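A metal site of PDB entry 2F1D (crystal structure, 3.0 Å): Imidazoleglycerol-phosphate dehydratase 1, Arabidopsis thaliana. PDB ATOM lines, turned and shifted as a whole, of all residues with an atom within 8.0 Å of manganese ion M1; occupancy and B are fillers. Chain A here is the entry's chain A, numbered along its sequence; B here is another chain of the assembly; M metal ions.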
ATOM      1  N   PHE A  44     -13.484  -4.929  -6.532  1.00  0.00           N
ATOM      2  CA  PHE A  44     -12.046  -4.833  -6.755  1.00  0.00           C
ATOM      3  C   PHE A  44     -11.658  -5.328  -8.136  1.00  0.00           C
ATOM      4  O   PHE A  44     -10.761  -4.753  -8.741  1.00  0.00           O
ATOM      5  CB  PHE A  44     -11.227  -5.581  -5.693  1.00  0.00           C
ATOM      6  CG  PHE A  44      -9.764  -5.232  -5.743  1.00  0.00           C
ATOM      7  CD1 PHE A  44      -9.321  -4.063  -5.166  1.00  0.00           C
ATOM      8  CD2 PHE A  44      -8.856  -6.042  -6.395  1.00  0.00           C
ATOM      9  CE1 PHE A  44      -8.004  -3.724  -5.214  1.00  0.00           C
ATOM     10  CE2 PHE A  44      -7.516  -5.691  -6.458  1.00  0.00           C
ATOM     11  CZ  PHE A  44      -7.090  -4.527  -5.864  1.00  0.00           C
ATOM     12  N   HIS A  47     -12.299  -2.494 -10.629  1.00  0.00           N
ATOM     13  CA  HIS A  47     -11.202  -1.551 -10.574  1.00  0.00           C
ATOM     14  C   HIS A  47     -10.037  -2.063 -11.391  1.00  0.00           C
ATOM     15  O   HIS A  47      -9.425  -1.290 -12.121  1.00  0.00           O
ATOM     16  CB  HIS A  47     -10.770  -1.347  -9.128  1.00  0.00           C
ATOM     17  CG  HIS A  47      -9.731  -0.284  -8.938  1.00  0.00           C
ATOM     18  ND1 HIS A  47      -9.878   0.992  -9.428  1.00  0.00           N
ATOM     19  CD2 HIS A  47      -8.544  -0.313  -8.295  1.00  0.00           C
ATOM     20  CE1 HIS A  47      -8.818   1.714  -9.099  1.00  0.00           C
ATOM     21  NE2 HIS A  47      -7.990   0.942  -8.404  1.00  0.00           N
ATOM     22  N   MET A  48      -9.750  -3.358 -11.304  1.00  0.00           N
ATOM     23  CA  MET A  48      -8.589  -3.939 -11.963  1.00  0.00           C
ATOM     24  C   MET A  48      -8.796  -4.027 -13.451  1.00  0.00           C
ATOM     25  O   MET A  48      -7.861  -3.845 -14.217  1.00  0.00           O
ATOM     26  CB  MET A  48      -8.284  -5.326 -11.418  1.00  0.00           C
ATOM     27  CG  MET A  48      -7.535  -5.290 -10.102  1.00  0.00           C
ATOM     28  SD  MET A  48      -6.185  -4.125 -10.121  1.00  0.00           S
ATOM     29  CE  MET A  48      -6.815  -2.902  -9.198  1.00  0.00           C
ATOM     30  N   GLN A  51      -8.341  -0.722 -15.078  1.00  0.00           N
ATOM     31  CA  GLN A  51      -6.918  -0.464 -15.305  1.00  0.00           C
ATOM     32  C   GLN A  51      -6.420  -1.180 -16.569  1.00  0.00           C
ATOM     33  O   GLN A  51      -5.630  -0.634 -17.324  1.00  0.00           O
ATOM     34  CB  GLN A  51      -6.080  -0.891 -14.101  1.00  0.00           C
ATOM     35  CG  GLN A  51      -6.419  -0.173 -12.799  1.00  0.00           C
ATOM     36  CD  GLN A  51      -5.862   1.253 -12.716  1.00  0.00           C
ATOM     37  OE1 GLN A  51      -4.671   1.488 -12.966  1.00  0.00           O
ATOM     38  NE2 GLN A  51      -6.719   2.192 -12.339  1.00  0.00           N
ATOM     39  N   LEU A 107       4.253   0.988  -9.361  1.00  0.00           N
ATOM     40  CA  LEU A 107       3.293   1.852  -8.693  1.00  0.00           C
ATOM     41  C   LEU A 107       3.786   2.063  -7.265  1.00  0.00           C
ATOM     42  O   LEU A 107       3.632   1.195  -6.403  1.00  0.00           O
ATOM     43  CB  LEU A 107       1.891   1.243  -8.717  1.00  0.00           C
ATOM     44  CG  LEU A 107       0.827   1.741  -7.725  1.00  0.00           C
ATOM     45  CD1 LEU A 107       0.854   3.226  -7.532  1.00  0.00           C
ATOM     46  CD2 LEU A 107      -0.543   1.305  -8.225  1.00  0.00           C
ATOM     47  N   HIS A 169      -2.560  -3.580  -2.567  1.00  0.00           N
ATOM     48  CA  HIS A 169      -3.360  -2.891  -3.574  1.00  0.00           C
ATOM     49  C   HIS A 169      -2.447  -2.354  -4.669  1.00  0.00           C
ATOM     50  O   HIS A 169      -2.852  -2.272  -5.824  1.00  0.00           O
ATOM     51  CB  HIS A 169      -4.165  -1.755  -2.909  1.00  0.00           C
ATOM     52  CG  HIS A 169      -5.066  -0.999  -3.847  1.00  0.00           C
ATOM     53  ND1 HIS A 169      -6.261  -1.500  -4.308  1.00  0.00           N
ATOM     54  CD2 HIS A 169      -4.974   0.254  -4.358  1.00  0.00           C
ATOM     55  CE1 HIS A 169      -6.852  -0.611  -5.086  1.00  0.00           C
ATOM     56  NE2 HIS A 169      -6.085   0.457  -5.135  1.00  0.00           N
ATOM     57  N   HIS A 170      -1.213  -2.023  -4.292  1.00  0.00           N
ATOM     58  CA  HIS A 170      -0.204  -1.532  -5.230  1.00  0.00           C
ATOM     59  C   HIS A 170       0.425  -2.634  -6.053  1.00  0.00           C
ATOM     60  O   HIS A 170       0.811  -2.389  -7.184  1.00  0.00           O
ATOM     61  CB  HIS A 170       0.928  -0.854  -4.485  1.00  0.00           C
ATOM     62  CG  HIS A 170       0.587   0.513  -3.997  1.00  0.00           C
ATOM     63  ND1 HIS A 170       1.464   1.263  -3.255  1.00  0.00           N
ATOM     64  CD2 HIS A 170      -0.528   1.251  -4.127  1.00  0.00           C
ATOM     65  CE1 HIS A 170       0.910   2.423  -2.960  1.00  0.00           C
ATOM     66  NE2 HIS A 170      -0.309   2.442  -3.473  1.00  0.00           N
ATOM     67  N   GLU A 173      -2.308  -3.937  -8.592  1.00  0.00           N
ATOM     68  CA  GLU A 173      -2.615  -2.910  -9.571  1.00  0.00           C
ATOM     69  C   GLU A 173      -1.481  -2.706 -10.587  1.00  0.00           C
ATOM     70  O   GLU A 173      -1.711  -2.520 -11.785  1.00  0.00           O
ATOM     71  CB  GLU A 173      -2.900  -1.602  -8.855  1.00  0.00           C
ATOM     72  CG  GLU A 173      -3.313  -0.450  -9.764  1.00  0.00           C
ATOM     73  CD  GLU A 173      -4.305   0.471  -9.109  1.00  0.00           C
ATOM     74  OE1 GLU A 173      -4.919   0.077  -8.093  1.00  0.00           O
ATOM     75  OE2 GLU A 173      -4.469   1.594  -9.625  1.00  0.00           O
ATOM     76  N   LYS A 177      -1.469  -3.079 -14.688  1.00  0.00           N
ATOM     77  CA  LYS A 177      -0.942  -2.013 -15.525  1.00  0.00           C
ATOM     78  C   LYS A 177       0.084  -2.579 -16.494  1.00  0.00           C
ATOM     79  O   LYS A 177       0.107  -2.216 -17.656  1.00  0.00           O
ATOM     80  CB  LYS A 177      -0.290  -0.910 -14.686  1.00  0.00           C
ATOM     81  CG  LYS A 177      -1.274   0.060 -14.079  1.00  0.00           C
ATOM     82  CD  LYS A 177      -0.599   1.122 -13.212  1.00  0.00           C
ATOM     83  CE  LYS A 177      -1.653   1.977 -12.512  1.00  0.00           C
ATOM     84  NZ  LYS A 177      -1.141   2.929 -11.476  1.00  0.00           N
ATOM     85  N   GLU B  21     -12.025   9.495  -8.145  1.00  0.00           N
ATOM     86  CA  GLU B  21     -12.291   8.542  -7.067  1.00  0.00           C
ATOM     87  C   GLU B  21     -12.933   9.166  -5.804  1.00  0.00           C
ATOM     88  O   GLU B  21     -13.937   8.648  -5.308  1.00  0.00           O
ATOM     89  CB  GLU B  21     -10.992   7.821  -6.700  1.00  0.00           C
ATOM     90  CG  GLU B  21     -10.573   6.755  -7.728  1.00  0.00           C
ATOM     91  CD  GLU B  21      -9.195   7.000  -8.343  1.00  0.00           C
ATOM     92  OE1 GLU B  21      -8.887   8.164  -8.673  1.00  0.00           O
ATOM     93  OE2 GLU B  21      -8.431   6.015  -8.513  1.00  0.00           O
ATOM     94  N   ASP B  67     -14.340   5.645  -2.955  1.00  0.00           N
ATOM     95  CA  ASP B  67     -14.539   4.246  -3.362  1.00  0.00           C
ATOM     96  C   ASP B  67     -14.706   3.245  -2.229  1.00  0.00           C
ATOM     97  O   ASP B  67     -14.412   2.064  -2.422  1.00  0.00           O
ATOM     98  CB  ASP B  67     -13.325   3.686  -4.115  1.00  0.00           C
ATOM     99  CG  ASP B  67     -12.822   4.587  -5.157  1.00  0.00           C
ATOM    100  OD1 ASP B  67     -13.088   4.303  -6.347  1.00  0.00           O
ATOM    101  OD2 ASP B  67     -12.080   5.544  -4.879  1.00  0.00           O
ATOM    102  N   ILE B  70     -14.958  -0.505  -3.122  1.00  0.00           N
ATOM    103  CA  ILE B  70     -13.810  -1.298  -3.609  1.00  0.00           C
ATOM    104  C   ILE B  70     -12.896  -1.643  -2.446  1.00  0.00           C
ATOM    105  O   ILE B  70     -12.787  -2.799  -2.028  1.00  0.00           O
ATOM    106  CB  ILE B  70     -12.913  -0.526  -4.626  1.00  0.00           C
ATOM    107  CG1 ILE B  70     -13.675  -0.047  -5.866  1.00  0.00           C
ATOM    108  CG2 ILE B  70     -11.731  -1.391  -5.011  1.00  0.00           C
ATOM    109  CD1 ILE B  70     -12.897   0.987  -6.685  1.00  0.00           C
ATOM    110  N   ASP B  71     -12.272  -0.577  -1.917  1.00  0.00           N
ATOM    111  CA  ASP B  71     -11.142  -0.594  -0.996  1.00  0.00           C
ATOM    112  C   ASP B  71     -11.391   0.539  -0.005  1.00  0.00           C
ATOM    113  O   ASP B  71     -12.370   1.250  -0.120  1.00  0.00           O
ATOM    114  CB  ASP B  71      -9.884  -0.250  -1.788  1.00  0.00           C
ATOM    115  CG  ASP B  71      -8.694  -1.054  -1.367  1.00  0.00           C
ATOM    116  OD1 ASP B  71      -8.812  -1.864  -0.433  1.00  0.00           O
ATOM    117  OD2 ASP B  71      -7.578  -0.950  -1.929  1.00  0.00           O
ATOM    118  N   HIS B  73      -8.469   2.198   0.270  1.00  0.00           N
ATOM    119  CA  HIS B  73      -7.167   2.727  -0.164  1.00  0.00           C
ATOM    120  C   HIS B  73      -7.173   4.144  -0.770  1.00  0.00           C
ATOM    121  O   HIS B  73      -6.333   4.959  -0.433  1.00  0.00           O
ATOM    122  CB  HIS B  73      -6.538   1.756  -1.165  1.00  0.00           C
ATOM    123  CG  HIS B  73      -5.100   2.052  -1.475  1.00  0.00           C
ATOM    124  ND1 HIS B  73      -4.071   1.364  -0.881  1.00  0.00           N
ATOM    125  CD2 HIS B  73      -4.533   2.967  -2.285  1.00  0.00           C
ATOM    126  CE1 HIS B  73      -2.920   1.852  -1.330  1.00  0.00           C
ATOM    127  NE2 HIS B  73      -3.180   2.815  -2.181  1.00  0.00           N
ATOM    128  N   HIS B  74      -8.097   4.387  -1.683  1.00  0.00           N
ATOM    129  CA  HIS B  74      -8.163   5.639  -2.430  1.00  0.00           C
ATOM    130  C   HIS B  74      -8.592   6.817  -1.577  1.00  0.00           C
ATOM    131  O   HIS B  74      -8.098   7.926  -1.753  1.00  0.00           O
ATOM    132  CB  HIS B  74      -9.136   5.521  -3.585  1.00  0.00           C
ATOM    133  CG  HIS B  74      -8.742   4.520  -4.625  1.00  0.00           C
ATOM    134  ND1 HIS B  74      -9.642   3.981  -5.511  1.00  0.00           N
ATOM    135  CD2 HIS B  74      -7.546   3.968  -4.919  1.00  0.00           C
ATOM    136  CE1 HIS B  74      -9.019   3.132  -6.311  1.00  0.00           C
ATOM    137  NE2 HIS B  74      -7.746   3.104  -5.974  1.00  0.00           N
ATOM    138  N   GLU B  77      -5.759   7.718   1.032  1.00  0.00           N
ATOM    139  CA  GLU B  77      -4.608   8.410   0.474  1.00  0.00           C
ATOM    140  C   GLU B  77      -4.948   9.839   0.032  1.00  0.00           C
ATOM    141  O   GLU B  77      -4.142  10.749   0.230  1.00  0.00           O
ATOM    142  CB  GLU B  77      -4.017   7.605  -0.708  1.00  0.00           C
ATOM    143  CG  GLU B  77      -3.315   8.473  -1.761  1.00  0.00           C
ATOM    144  CD  GLU B  77      -2.447   7.671  -2.703  1.00  0.00           C
ATOM    145  OE1 GLU B  77      -2.710   6.453  -2.886  1.00  0.00           O
ATOM    146  OE2 GLU B  77      -1.499   8.270  -3.264  1.00  0.00           O
HETATM  147 MN    MN M   1      -6.271   1.912  -7.187  1.00  0.00          MN
HETATM  148 MN    MN M   2      -1.590   4.436  -3.254  1.00  0.00          MN
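OD2 of Asp 67 of chain B lies within hydrogen-bond range of ND1 of His 74 of chain B (3.0 Å).
OE1 of Gln 51 sits close to OE2 of Glu 173, 3.3 Å away.
ND1 of His 169 is in hydrogen-bond range of OD2 of Asp 71 of chain B (2.8 Å).
Four residues have an atom within 4 Å of manganese ion M1: His 47, His 169, Glu 173 and His 74 of chain B.
Manganese ion M1 is bound by a ring nitrogen (NE2) of His 74 of chain B (2.3 Å), a ring nitrogen (NE2) of His 47 (2.3 Å), the side-chain carboxylate (OE1) of Glu 173 (2.5 Å) and a ring nitrogen (NE2) of His 169 (2.5 Å).
Manganese ion M1 has four donor atoms within binding distance.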
